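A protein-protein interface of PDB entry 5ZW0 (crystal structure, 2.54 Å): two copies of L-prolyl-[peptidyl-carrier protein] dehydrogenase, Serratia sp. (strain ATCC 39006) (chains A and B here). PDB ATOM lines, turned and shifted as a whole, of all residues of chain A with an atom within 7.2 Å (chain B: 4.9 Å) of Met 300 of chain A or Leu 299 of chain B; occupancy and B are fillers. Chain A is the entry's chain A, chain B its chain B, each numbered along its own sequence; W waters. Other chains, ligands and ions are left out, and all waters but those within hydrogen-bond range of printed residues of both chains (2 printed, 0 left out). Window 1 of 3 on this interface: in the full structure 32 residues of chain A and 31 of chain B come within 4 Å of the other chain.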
ATOM      1  N   MET A   1     -23.703   5.119  11.857  1.00  0.00           N
ATOM      2  CA  MET A   1     -23.432   3.896  11.109  1.00  0.00           C
ATOM      3  C   MET A   1     -22.620   4.099   9.821  1.00  0.00           C
ATOM      4  O   MET A   1     -23.000   4.861   8.957  1.00  0.00           O
ATOM      5  CB  MET A   1     -24.748   3.223  10.763  1.00  0.00           C
ATOM      6  CG  MET A   1     -24.611   1.738  10.575  1.00  0.00           C
ATOM      7  SD  MET A   1     -25.329   0.875  11.966  1.00  0.00           S
ATOM      8  CE  MET A   1     -27.026   1.063  11.485  1.00  0.00           C
ATOM      9  N   PHE A   3     -19.874   1.681   7.117  1.00  0.00           N
ATOM     10  CA  PHE A   3     -19.367   0.353   6.800  1.00  0.00           C
ATOM     11  C   PHE A   3     -18.162   0.413   5.876  1.00  0.00           C
ATOM     12  O   PHE A   3     -17.793  -0.599   5.258  1.00  0.00           O
ATOM     13  CB  PHE A   3     -20.474  -0.506   6.181  1.00  0.00           C
ATOM     14  CG  PHE A   3     -21.571  -0.833   7.136  1.00  0.00           C
ATOM     15  CD1 PHE A   3     -21.456  -1.914   8.003  1.00  0.00           C
ATOM     16  CD2 PHE A   3     -22.726  -0.046   7.182  1.00  0.00           C
ATOM     17  CE1 PHE A   3     -22.474  -2.209   8.914  1.00  0.00           C
ATOM     18  CE2 PHE A   3     -23.753  -0.342   8.065  1.00  0.00           C
ATOM     19  CZ  PHE A   3     -23.631  -1.423   8.939  1.00  0.00           C
ATOM     20  N   LEU A 294     -19.340 -15.693   5.477  1.00  0.00           N
ATOM     21  CA  LEU A 294     -18.204 -14.792   5.580  1.00  0.00           C
ATOM     22  C   LEU A 294     -18.666 -13.387   5.943  1.00  0.00           C
ATOM     23  O   LEU A 294     -18.146 -12.776   6.885  1.00  0.00           O
ATOM     24  CB  LEU A 294     -17.432 -14.780   4.265  1.00  0.00           C
ATOM     25  CG  LEU A 294     -16.251 -13.777   4.215  1.00  0.00           C
ATOM     26  CD1 LEU A 294     -15.155 -14.143   5.197  1.00  0.00           C
ATOM     27  CD2 LEU A 294     -15.668 -13.727   2.835  1.00  0.00           C
ATOM     28  N   GLU A 295     -19.673 -12.873   5.233  1.00  0.00           N
ATOM     29  CA  GLU A 295     -20.131 -11.510   5.508  1.00  0.00           C
ATOM     30  C   GLU A 295     -20.747 -11.384   6.901  1.00  0.00           C
ATOM     31  O   GLU A 295     -20.454 -10.422   7.631  1.00  0.00           O
ATOM     32  CB  GLU A 295     -21.108 -11.071   4.431  1.00  0.00           C
ATOM     33  CG  GLU A 295     -20.456 -11.029   3.067  1.00  0.00           C
ATOM     34  CD  GLU A 295     -19.258 -10.098   3.016  1.00  0.00           C
ATOM     35  OE1 GLU A 295     -19.382  -8.923   3.379  1.00  0.00           O
ATOM     36  OE2 GLU A 295     -18.175 -10.534   2.607  1.00  0.00           O
ATOM     37  N   GLN A 296     -21.578 -12.354   7.307  1.00  0.00           N
ATOM     38  CA  GLN A 296     -22.218 -12.249   8.615  1.00  0.00           C
ATOM     39  C   GLN A 296     -21.193 -12.238   9.736  1.00  0.00           C
ATOM     40  O   GLN A 296     -21.207 -11.359  10.612  1.00  0.00           O
ATOM     41  CB  GLN A 296     -23.181 -13.402   8.812  1.00  0.00           C
ATOM     42  CG  GLN A 296     -24.482 -13.289   8.056  1.00  0.00           C
ATOM     43  CD  GLN A 296     -25.257 -14.557   8.233  1.00  0.00           C
ATOM     44  OE1 GLN A 296     -24.848 -15.615   7.737  1.00  0.00           O
ATOM     45  NE2 GLN A 296     -26.330 -14.495   9.013  1.00  0.00           N
ATOM     46  N   CYS A 297     -20.290 -13.210   9.739  1.00  0.00           N
ATOM     47  CA  CYS A 297     -19.416 -13.267  10.890  1.00  0.00           C
ATOM     48  C   CYS A 297     -18.307 -12.216  10.791  1.00  0.00           C
ATOM     49  O   CYS A 297     -17.843 -11.703  11.806  1.00  0.00           O
ATOM     50  CB  CYS A 297     -18.886 -14.689  11.066  1.00  0.00           C
ATOM     51  SG  CYS A 297     -17.707 -15.209   9.851  1.00  0.00           S
ATOM     52  N   ARG A 298     -17.929 -11.811   9.594  1.00  0.00           N
ATOM     53  CA  ARG A 298     -17.054 -10.655   9.454  1.00  0.00           C
ATOM     54  C   ARG A 298     -17.640  -9.433  10.169  1.00  0.00           C
ATOM     55  O   ARG A 298     -16.973  -8.799  10.995  1.00  0.00           O
ATOM     56  CB  ARG A 298     -16.871 -10.395   7.957  1.00  0.00           C
ATOM     57  CG  ARG A 298     -16.152  -9.184   7.672  1.00  0.00           C
ATOM     58  CD  ARG A 298     -15.061  -9.413   6.659  1.00  0.00           C
ATOM     59  NE  ARG A 298     -15.577  -9.662   5.326  1.00  0.00           N
ATOM     60  CZ  ARG A 298     -14.801 -10.021   4.320  1.00  0.00           C
ATOM     61  NH1 ARG A 298     -15.325 -10.244   3.117  1.00  0.00           N
ATOM     62  NH2 ARG A 298     -13.499 -10.177   4.525  1.00  0.00           N
ATOM     63  N   LEU A 299     -18.909  -9.108   9.885  1.00  0.00           N
ATOM     64  CA  LEU A 299     -19.505  -7.944  10.526  1.00  0.00           C
ATOM     65  C   LEU A 299     -19.633  -8.137  12.044  1.00  0.00           C
ATOM     66  O   LEU A 299     -19.451  -7.187  12.815  1.00  0.00           O
ATOM     67  CB  LEU A 299     -20.859  -7.634   9.904  1.00  0.00           C
ATOM     68  CG  LEU A 299     -20.831  -7.211   8.437  1.00  0.00           C
ATOM     69  CD1 LEU A 299     -22.260  -7.019   7.893  1.00  0.00           C
ATOM     70  CD2 LEU A 299     -20.044  -5.964   8.267  1.00  0.00           C
ATOM     71  N   MET A 300     -19.964  -9.346  12.500  1.00  0.00           N
ATOM     72  CA  MET A 300     -20.035  -9.560  13.947  1.00  0.00           C
ATOM     73  C   MET A 300     -18.685  -9.290  14.612  1.00  0.00           C
ATOM     74  O   MET A 300     -18.614  -8.689  15.703  1.00  0.00           O
ATOM     75  CB  MET A 300     -20.504 -10.985  14.248  1.00  0.00           C
ATOM     76  CG  MET A 300     -21.920 -11.269  13.842  1.00  0.00           C
ATOM     77  SD  MET A 300     -23.105 -10.290  14.787  1.00  0.00           S
ATOM     78  CE  MET A 300     -23.137 -11.203  16.340  1.00  0.00           C
ATOM     79  N   LEU A 301     -17.599  -9.708  13.956  1.00  0.00           N
ATOM     80  CA  LEU A 301     -16.269  -9.519  14.523  1.00  0.00           C
ATOM     81  C   LEU A 301     -15.875  -8.044  14.530  1.00  0.00           C
ATOM     82  O   LEU A 301     -15.350  -7.530  15.528  1.00  0.00           O
ATOM     83  CB  LEU A 301     -15.242 -10.338  13.739  1.00  0.00           C
ATOM     84  CG  LEU A 301     -13.795 -10.040  14.175  1.00  0.00           C
ATOM     85  CD1 LEU A 301     -13.553 -10.506  15.603  1.00  0.00           C
ATOM     86  CD2 LEU A 301     -12.792 -10.642  13.241  1.00  0.00           C
ATOM     87  N   TYR A 302     -16.079  -7.352  13.408  1.00  0.00           N
ATOM     88  CA  TYR A 302     -15.735  -5.934  13.376  1.00  0.00           C
ATOM     89  C   TYR A 302     -16.481  -5.181  14.457  1.00  0.00           C
ATOM     90  O   TYR A 302     -15.924  -4.274  15.079  1.00  0.00           O
ATOM     91  CB  TYR A 302     -16.059  -5.315  12.018  1.00  0.00           C
ATOM     92  CG  TYR A 302     -15.271  -5.896  10.908  1.00  0.00           C
ATOM     93  CD1 TYR A 302     -14.091  -6.596  11.161  1.00  0.00           C
ATOM     94  CD2 TYR A 302     -15.698  -5.771   9.604  1.00  0.00           C
ATOM     95  CE1 TYR A 302     -13.358  -7.137  10.141  1.00  0.00           C
ATOM     96  CE2 TYR A 302     -14.975  -6.314   8.577  1.00  0.00           C
ATOM     97  CZ  TYR A 302     -13.810  -6.997   8.848  1.00  0.00           C
ATOM     98  OH  TYR A 302     -13.097  -7.528   7.818  1.00  0.00           O
ATOM     99  N   ARG A 303     -17.758  -5.514  14.669  1.00  0.00           N
ATOM    100  CA  ARG A 303     -18.529  -4.752  15.637  1.00  0.00           C
ATOM    101  C   ARG A 303     -18.054  -5.042  17.047  1.00  0.00           C
ATOM    102  O   ARG A 303     -17.938  -4.126  17.859  1.00  0.00           O
ATOM    103  CB  ARG A 303     -20.024  -5.044  15.491  1.00  0.00           C
ATOM    104  CG  ARG A 303     -20.888  -4.123  16.339  1.00  0.00           C
ATOM    105  CD  ARG A 303     -22.356  -4.413  16.193  1.00  0.00           C
ATOM    106  NE  ARG A 303     -22.767  -5.527  17.046  1.00  0.00           N
ATOM    107  CZ  ARG A 303     -23.970  -6.097  16.995  1.00  0.00           C
ATOM    108  NH1 ARG A 303     -24.862  -5.657  16.130  1.00  0.00           N
ATOM    109  NH2 ARG A 303     -24.287  -7.101  17.806  1.00  0.00           N
ATOM    110  N   ALA A 304     -17.773  -6.306  17.371  1.00  0.00           N
ATOM    111  CA  ALA A 304     -17.185  -6.572  18.676  1.00  0.00           C
ATOM    112  C   ALA A 304     -15.896  -5.762  18.865  1.00  0.00           C
ATOM    113  O   ALA A 304     -15.703  -5.098  19.899  1.00  0.00           O
ATOM    114  CB  ALA A 304     -16.938  -8.064  18.841  1.00  0.00           C
ATOM    115  N   CYS A 305     -15.006  -5.782  17.862  1.00  0.00           N
ATOM    116  CA  CYS A 305     -13.747  -5.047  18.008  1.00  0.00           C
ATOM    117  C   CYS A 305     -13.994  -3.555  18.157  1.00  0.00           C
ATOM    118  O   CYS A 305     -13.408  -2.899  19.031  1.00  0.00           O
ATOM    119  CB  CYS A 305     -12.814  -5.327  16.831  1.00  0.00           C
ATOM    120  SG  CYS A 305     -12.231  -7.017  16.925  1.00  0.00           S
ATOM    121  N   TRP A 306     -14.894  -3.014  17.347  1.00  0.00           N
ATOM    122  CA  TRP A 306     -15.215  -1.599  17.420  1.00  0.00           C
ATOM    123  C   TRP A 306     -15.787  -1.236  18.784  1.00  0.00           C
ATOM    124  O   TRP A 306     -15.379  -0.236  19.382  1.00  0.00           O
ATOM    125  CB  TRP A 306     -16.193  -1.260  16.312  1.00  0.00           C
ATOM    126  CG  TRP A 306     -16.721   0.145  16.369  1.00  0.00           C
ATOM    127  CD1 TRP A 306     -16.140   1.265  15.831  1.00  0.00           C
ATOM    128  CD2 TRP A 306     -17.955   0.576  16.960  1.00  0.00           C
ATOM    129  NE1 TRP A 306     -16.921   2.365  16.082  1.00  0.00           N
ATOM    130  CE2 TRP A 306     -18.041   1.970  16.771  1.00  0.00           C
ATOM    131  CE3 TRP A 306     -18.983  -0.076  17.659  1.00  0.00           C
ATOM    132  CZ2 TRP A 306     -19.134   2.725  17.242  1.00  0.00           C
ATOM    133  CZ3 TRP A 306     -20.061   0.674  18.124  1.00  0.00           C
ATOM    134  CH2 TRP A 306     -20.132   2.052  17.903  1.00  0.00           C
ATOM    135  N   ALA A 316     -19.445 -10.378  25.347  1.00  0.00           N
ATOM    136  CA  ALA A 316     -20.461 -11.220  24.721  1.00  0.00           C
ATOM    137  C   ALA A 316     -20.415 -11.114  23.196  1.00  0.00           C
ATOM    138  O   ALA A 316     -20.640 -12.102  22.488  1.00  0.00           O
ATOM    139  CB  ALA A 316     -21.838 -10.857  25.258  1.00  0.00           C
ATOM    140  N   ASP A 317     -20.121  -9.927  22.670  1.00  0.00           N
ATOM    141  CA  ASP A 317     -19.974  -9.783  21.231  1.00  0.00           C
ATOM    142  C   ASP A 317     -18.808 -10.601  20.703  1.00  0.00           C
ATOM    143  O   ASP A 317     -18.895 -11.199  19.625  1.00  0.00           O
ATOM    144  CB  ASP A 317     -19.794  -8.316  20.888  1.00  0.00           C
ATOM    145  CG  ASP A 317     -21.073  -7.558  21.033  1.00  0.00           C
ATOM    146  OD1 ASP A 317     -21.868  -7.583  20.051  1.00  0.00           O
ATOM    147  OD2 ASP A 317     -21.279  -6.987  22.136  1.00  0.00           O
ATOM    148  N   ILE A 318     -17.707 -10.634  21.448  1.00  0.00           N
ATOM    149  CA  ILE A 318     -16.561 -11.426  21.031  1.00  0.00           C
ATOM    150  C   ILE A 318     -16.887 -12.902  21.142  1.00  0.00           C
ATOM    151  O   ILE A 318     -16.510 -13.694  20.278  1.00  0.00           O
ATOM    152  CB  ILE A 318     -15.312 -11.041  21.854  1.00  0.00           C
ATOM    153  CG1 ILE A 318     -14.511  -9.997  21.110  1.00  0.00           C
ATOM    154  CG2 ILE A 318     -14.394 -12.197  22.004  1.00  0.00           C
ATOM    155  CD1 ILE A 318     -13.895 -10.580  19.833  1.00  0.00           C
ATOM    156  N   MET A 320     -19.865 -14.213  20.681  1.00  0.00           N
ATOM    157  CA  MET A 320     -20.684 -14.473  19.502  1.00  0.00           C
ATOM    158  C   MET A 320     -19.822 -14.583  18.246  1.00  0.00           C
ATOM    159  O   MET A 320     -20.079 -15.423  17.378  1.00  0.00           O
ATOM    160  CB  MET A 320     -21.745 -13.371  19.344  1.00  0.00           C
ATOM    161  CG  MET A 320     -22.846 -13.322  20.414  1.00  0.00           C
ATOM    162  SD  MET A 320     -24.212 -12.163  20.033  1.00  0.00           S
ATOM    163  CE  MET A 320     -23.369 -10.593  20.022  1.00  0.00           C
ATOM    164  N   SER A 321     -18.819 -13.716  18.111  1.00  0.00           N
ATOM    165  CA  SER A 321     -17.947 -13.784  16.947  1.00  0.00           C
ATOM    166  C   SER A 321     -17.218 -15.116  16.890  1.00  0.00           C
ATOM    167  O   SER A 321     -17.163 -15.761  15.840  1.00  0.00           O
ATOM    168  CB  SER A 321     -16.949 -12.637  16.963  1.00  0.00           C
ATOM    169  OG  SER A 321     -17.631 -11.469  16.612  1.00  0.00           O
ATOM    170  N   LYS A 322     -16.625 -15.522  18.008  1.00  0.00           N
ATOM    171  CA  LYS A 322     -15.876 -16.761  18.015  1.00  0.00           C
ATOM    172  C   LYS A 322     -16.793 -17.935  17.703  1.00  0.00           C
ATOM    173  O   LYS A 322     -16.444 -18.819  16.918  1.00  0.00           O
ATOM    174  CB  LYS A 322     -15.194 -16.941  19.370  1.00  0.00           C
ATOM    175  CG  LYS A 322     -14.210 -18.104  19.388  1.00  0.00           C
ATOM    176  CD  LYS A 322     -14.831 -19.298  20.089  1.00  0.00           C
ATOM    177  CE  LYS A 322     -14.047 -20.589  19.833  1.00  0.00           C
ATOM    178  NZ  LYS A 322     -14.869 -21.836  20.075  1.00  0.00           N
ATOM    179  N   LEU A 324     -19.693 -18.039  15.981  1.00  0.00           N
ATOM    180  CA  LEU A 324     -20.079 -18.032  14.582  1.00  0.00           C
ATOM    181  C   LEU A 324     -18.927 -18.442  13.684  1.00  0.00           C
ATOM    182  O   LEU A 324     -19.117 -19.229  12.753  1.00  0.00           O
ATOM    183  CB  LEU A 324     -20.584 -16.640  14.195  1.00  0.00           C
ATOM    184  CG  LEU A 324     -21.958 -16.274  14.755  1.00  0.00           C
ATOM    185  CD1 LEU A 324     -22.299 -14.816  14.434  1.00  0.00           C
ATOM    186  CD2 LEU A 324     -23.044 -17.242  14.205  1.00  0.00           C
ATOM    187  N   ILE A 325     -17.723 -17.928  13.952  1.00  0.00           N
ATOM    188  CA  ILE A 325     -16.597 -18.164  13.054  1.00  0.00           C
ATOM    189  C   ILE A 325     -16.129 -19.605  13.139  1.00  0.00           C
ATOM    190  O   ILE A 325     -15.832 -20.223  12.116  1.00  0.00           O
ATOM    191  CB  ILE A 325     -15.454 -17.168  13.341  1.00  0.00           C
ATOM    192  CG1 ILE A 325     -15.864 -15.763  12.880  1.00  0.00           C
ATOM    193  CG2 ILE A 325     -14.154 -17.609  12.657  1.00  0.00           C
ATOM    194  CD1 ILE A 325     -15.159 -14.625  13.605  1.00  0.00           C
ATOM    195  N   PHE B   3     -20.574   1.508  14.392  1.00  0.00           N
ATOM    196  CA  PHE B   3     -21.718   0.619  14.540  1.00  0.00           C
ATOM    197  C   PHE B   3     -22.785   1.196  15.455  1.00  0.00           C
ATOM    198  O   PHE B   3     -23.639   0.452  15.961  1.00  0.00           O
ATOM    199  CB  PHE B   3     -21.272  -0.766  15.027  1.00  0.00           C
ATOM    200  CG  PHE B   3     -20.478  -1.541  14.003  1.00  0.00           C
ATOM    201  CD1 PHE B   3     -21.119  -2.299  13.047  1.00  0.00           C
ATOM    202  CD2 PHE B   3     -19.093  -1.508  13.999  1.00  0.00           C
ATOM    203  CE1 PHE B   3     -20.402  -3.011  12.105  1.00  0.00           C
ATOM    204  CE2 PHE B   3     -18.382  -2.215  13.073  1.00  0.00           C
ATOM    205  CZ  PHE B   3     -19.038  -2.978  12.118  1.00  0.00           C
ATOM    206  N   LEU B 294     -30.555 -12.731  14.918  1.00  0.00           N
ATOM    207  CA  LEU B 294     -31.019 -11.361  14.856  1.00  0.00           C
ATOM    208  C   LEU B 294     -29.850 -10.401  14.640  1.00  0.00           C
ATOM    209  O   LEU B 294     -29.898  -9.534  13.765  1.00  0.00           O
ATOM    210  CB  LEU B 294     -31.801 -11.034  16.126  1.00  0.00           C
ATOM    211  CG  LEU B 294     -32.158  -9.548  16.292  1.00  0.00           C
ATOM    212  CD1 LEU B 294     -33.098  -9.086  15.158  1.00  0.00           C
ATOM    213  CD2 LEU B 294     -32.749  -9.282  17.668  1.00  0.00           C
ATOM    214  N   GLU B 295     -28.782 -10.545  15.414  1.00  0.00           N
ATOM    215  CA  GLU B 295     -27.694  -9.591  15.254  1.00  0.00           C
ATOM    216  C   GLU B 295     -27.086  -9.681  13.854  1.00  0.00           C
ATOM    217  O   GLU B 295     -26.832  -8.648  13.210  1.00  0.00           O
ATOM    218  CB  GLU B 295     -26.639  -9.812  16.338  1.00  0.00           C
ATOM    219  CG  GLU B 295     -27.120  -9.575  17.773  1.00  0.00           C
ATOM    220  CD  GLU B 295     -27.690  -8.172  17.974  1.00  0.00           C
ATOM    221  OE1 GLU B 295     -27.011  -7.172  17.634  1.00  0.00           O
ATOM    222  OE2 GLU B 295     -28.841  -8.074  18.469  1.00  0.00           O
ATOM    223  N   GLN B 296     -26.894 -10.911  13.344  1.00  0.00           N
ATOM    224  CA  GLN B 296     -26.278 -11.093  12.032  1.00  0.00           C
ATOM    225  C   GLN B 296     -27.112 -10.470  10.921  1.00  0.00           C
ATOM    226  O   GLN B 296     -26.592  -9.736  10.065  1.00  0.00           O
ATOM    227  CB  GLN B 296     -26.091 -12.575  11.762  1.00  0.00           C
ATOM    228  CG  GLN B 296     -24.947 -13.181  12.492  1.00  0.00           C
ATOM    229  CD  GLN B 296     -24.904 -14.657  12.268  1.00  0.00           C
ATOM    230  OE1 GLN B 296     -24.049 -15.170  11.531  1.00  0.00           O
ATOM    231  NE2 GLN B 296     -25.830 -15.366  12.904  1.00  0.00           N
ATOM    232  N   CYS B 297     -28.406 -10.774  10.892  1.00  0.00           N
ATOM    233  CA  CYS B 297     -29.182 -10.285   9.762  1.00  0.00           C
ATOM    234  C   CYS B 297     -29.554  -8.820   9.930  1.00  0.00           C
ATOM    235  O   CYS B 297     -29.703  -8.104   8.941  1.00  0.00           O
ATOM    236  CB  CYS B 297     -30.397 -11.191   9.519  1.00  0.00           C
ATOM    237  SG  CYS B 297     -31.663 -11.172  10.729  1.00  0.00           S
ATOM    238  N   ARG B 298     -29.629  -8.331  11.158  1.00  0.00           N
ATOM    239  CA  ARG B 298     -29.709  -6.891  11.384  1.00  0.00           C
ATOM    240  C   ARG B 298     -28.530  -6.171  10.731  1.00  0.00           C
ATOM    241  O   ARG B 298     -28.721  -5.216   9.969  1.00  0.00           O
ATOM    242  CB  ARG B 298     -29.778  -6.646  12.893  1.00  0.00           C
ATOM    243  CG  ARG B 298     -29.729  -5.221  13.340  1.00  0.00           C
ATOM    244  CD  ARG B 298     -30.849  -4.887  14.366  1.00  0.00           C
ATOM    245  NE  ARG B 298     -30.644  -5.540  15.651  1.00  0.00           N
ATOM    246  CZ  ARG B 298     -31.557  -5.582  16.610  1.00  0.00           C
ATOM    247  NH1 ARG B 298     -31.286  -6.210  17.751  1.00  0.00           N
ATOM    248  NH2 ARG B 298     -32.747  -5.014  16.426  1.00  0.00           N
ATOM    249  N   LEU B 299     -27.299  -6.651  10.978  1.00  0.00           N
ATOM    250  CA  LEU B 299     -26.122  -5.983  10.407  1.00  0.00           C
ATOM    251  C   LEU B 299     -26.102  -6.072   8.886  1.00  0.00           C
ATOM    252  O   LEU B 299     -25.745  -5.097   8.200  1.00  0.00           O
ATOM    253  CB  LEU B 299     -24.836  -6.598  10.962  1.00  0.00           C
ATOM    254  CG  LEU B 299     -24.611  -6.311  12.433  1.00  0.00           C
ATOM    255  CD1 LEU B 299     -23.457  -7.153  13.007  1.00  0.00           C
ATOM    256  CD2 LEU B 299     -24.323  -4.793  12.530  1.00  0.00           C
ATOM    257  N   MET B 300     -26.459  -7.243   8.342  1.00  0.00           N
ATOM    258  CA  MET B 300     -26.525  -7.378   6.897  1.00  0.00           C
ATOM    259  C   MET B 300     -27.521  -6.382   6.309  1.00  0.00           C
ATOM    260  O   MET B 300     -27.273  -5.764   5.260  1.00  0.00           O
ATOM    261  CB  MET B 300     -26.911  -8.826   6.539  1.00  0.00           C
ATOM    262  CG  MET B 300     -25.845  -9.859   6.886  1.00  0.00           C
ATOM    263  SD  MET B 300     -24.348  -9.586   5.893  1.00  0.00           S
ATOM    264  CE  MET B 300     -24.823 -10.350   4.320  1.00  0.00           C
ATOM    265  N   LEU B 301     -28.643  -6.181   6.995  1.00  0.00           N
ATOM    266  CA  LEU B 301     -29.671  -5.288   6.472  1.00  0.00           C
ATOM    267  C   LEU B 301     -29.207  -3.838   6.498  1.00  0.00           C
ATOM    268  O   LEU B 301     -29.355  -3.109   5.505  1.00  0.00           O
ATOM    269  CB  LEU B 301     -30.963  -5.477   7.260  1.00  0.00           C
ATOM    270  CG  LEU B 301     -31.998  -4.410   6.913  1.00  0.00           C
ATOM    271  CD1 LEU B 301     -32.442  -4.494   5.436  1.00  0.00           C
ATOM    272  CD2 LEU B 301     -33.184  -4.520   7.870  1.00  0.00           C
ATOM    273  N   TYR B 302     -28.646  -3.403   7.629  1.00  0.00           N
ATOM    274  CA  TYR B 302     -28.129  -2.041   7.715  1.00  0.00           C
ATOM    275  C   TYR B 302     -27.063  -1.797   6.660  1.00  0.00           C
ATOM    276  O   TYR B 302     -26.990  -0.710   6.083  1.00  0.00           O
ATOM    277  CB  TYR B 302     -27.545  -1.761   9.098  1.00  0.00           C
ATOM    278  CG  TYR B 302     -28.556  -1.889  10.187  1.00  0.00           C
ATOM    279  CD1 TYR B 302     -29.921  -1.818   9.901  1.00  0.00           C
ATOM    280  CD2 TYR B 302     -28.165  -2.121  11.499  1.00  0.00           C
ATOM    281  CE1 TYR B 302     -30.866  -1.964  10.890  1.00  0.00           C
ATOM    282  CE2 TYR B 302     -29.099  -2.257  12.495  1.00  0.00           C
ATOM    283  CZ  TYR B 302     -30.449  -2.190  12.176  1.00  0.00           C
ATOM    284  OH  TYR B 302     -31.387  -2.341  13.142  1.00  0.00           O
ATOM    285  N   ARG B 303     -26.198  -2.781   6.409  1.00  0.00           N
ATOM    286  CA  ARG B 303     -25.142  -2.517   5.435  1.00  0.00           C
ATOM    287  C   ARG B 303     -25.710  -2.396   4.031  1.00  0.00           C
ATOM    288  O   ARG B 303     -25.288  -1.524   3.275  1.00  0.00           O
ATOM    289  CB  ARG B 303     -24.045  -3.576   5.478  1.00  0.00           C
ATOM    290  CG  ARG B 303     -22.869  -3.200   4.596  1.00  0.00           C
ATOM    291  CD  ARG B 303     -21.780  -4.206   4.724  1.00  0.00           C
ATOM    292  NE  ARG B 303     -22.016  -5.378   3.914  1.00  0.00           N
ATOM    293  CZ  ARG B 303     -21.317  -6.507   4.025  1.00  0.00           C
ATOM    294  NH1 ARG B 303     -20.360  -6.602   4.934  1.00  0.00           N
ATOM    295  NH2 ARG B 303     -21.589  -7.544   3.241  1.00  0.00           N
HETATM  296  O   HOH W   1     -18.437  -3.911   5.859  1.00  0.00           O
HETATM  297  O   HOH W   2     -25.493  -7.475  20.547  1.00  0.00           O
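Among the printed residues, pairs that only touch across the chains: Met 1 of chain A with Tyr 302 of chain B (3.4 Å), Phe 3 of chain A with Phe 3 of chain B (3.9 Å), Phe 3 of chain A with Tyr 302 of chain B (3.8 Å), Phe 3 of chain A with Arg 303 of chain B (3.7 Å), Glu 295 of chain A with Met 300 of chain B (3.8 Å), Gln 296 of chain A with Met 300 of chain B (3.9 Å), Leu 299 of chain A with Leu 299 of chain B (3.99 Å), Leu 299 of chain A with Met 300 of chain B (3.9 Å), Leu 299 of chain A with Arg 303 of chain B (3.4 Å), Met 300 of chain A with Glu 295 of chain B (3.8 Å), Met 300 of chain A with Gln 296 of chain B (3.8 Å), Met 300 of chain A with Leu 299 of chain B (3.6 Å), Tyr 302 of chain A with Phe 3 of chain B (3.8 Å), Arg 303 of chain A with Phe 3 of chain B (3.5 Å), Arg 303 of chain A with Leu 299 of chain B (3.7 Å), Trp 306 of chain A with Phe 3 of chain B (3.4 Å) and Leu 324 of chain A with Gln 296 of chain B (3.4 Å).
Phe 3 of chain B touches its own counterpart, Phe 3 of chain A.
Glu 295 of chain A touches Arg 303 of chain B, and with the chains exchanged Arg 303 of chain A touches Glu 295 of chain B.
Leu 299 of chain A touches Met 300 of chain B, and with the chains exchanged Met 300 of chain A touches Leu 299 of chain B.
Of the 11 printed residues of chain B, 7 touch a printed residue of chain A.
Hydrophobic or aromatic side chains of chain B within 4 Å of the printed part of chain A: Phe 3, Leu 299, Met 300 and Tyr 302.
Of the 23 printed residues of chain A, 10 touch a printed residue of chain B.
Printed residues of chain A that touch a printed residue of chain B: Met 1, Phe 3, Glu 295, Gln 296, Leu 299, Met 300, Tyr 302, Arg 303, Trp 306 and Leu 324.
Along chain A the printed residues that touch a printed residue of chain B span positions 1 to 324.
Among the printed residues, 20 pairs touch across the chains.
Among the printed residues, Asp or Glu carboxylates within 4 Å of a Lys or Arg side-chain nitrogen of the other chain: Glu 295 of chain A with Arg 303 of chain B (2.6 Å) and Arg 303 of chain A with Glu 295 of chain B (2.7 Å).
OE2 of Glu 295 of chain B lies within salt-bridge range of NH1 of Arg 298 of chain B.
OG of Ser 321 of chain A sits at hydrogen-bond distance from O of Met 300 of chain A (3.1 Å).
NH2 of Arg 303 of chain A is in salt-bridge range of OD1 of Asp 317 of chain A, at 3.3 Å.
The guanidinium group (NH1) of Arg 298 of chain A is in salt-bridge range of the side-chain carboxylate (OE2) of Glu 295 of chain A, 2.9 Å away.
The guanidinium group (NH2) of Arg 303 of chain A is in salt-bridge range of the side-chain carboxylate (OE1) of Glu 295 of chain B, 2.7 Å away.
The side-chain amide nitrogen (NE2) of Gln 296 of chain A sits close to the side-chain amide oxygen (OE1) of Gln 296 of chain B (3.5 Å).
NH2 of Arg 303 of chain B lies within salt-bridge range of OE1 of Glu 295 of chain A (2.6 Å).
Water W2 lies within hydrogen-bond range of NH2 of Arg 303 of chain A and OE1 of Glu 295 of chain B.
Water W1 bridges the backbone carbonyl oxygen of Phe 3 of chain A and the guanidinium group of Arg 303 of chain B.
Of chain B, only Glu 295 (3.8 Å), Gln 296 (3.8 Å) and Leu 299 (3.6 Å) come within 4 Å of Met 300 of chain A.
Printed residues of chain B within 4 Å of Tyr 302 of chain A: Phe 3.
Met 320 of chain A touches none of the printed residues of chain B.
Printed residues of chain A within 4 Å of Phe 3 of chain B: Phe 3 (3.9 Å), Tyr 302 (3.8 Å), Arg 303 (3.5 Å) and Trp 306 (3.4 Å).
Of the printed residues of chain A, Leu 299 of chain B touches Leu 299 (3.99 Å), Met 300 (3.6 Å) and Arg 303 (3.7 Å).
The nearest printed residue of chain B that does not touch Met 300 of chain A is Phe 3 of chain B (6.4 Å).
The nearest printed residue of chain A that does not touch Tyr 302 of chain B is Arg 303 of chain A (6.5 Å).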
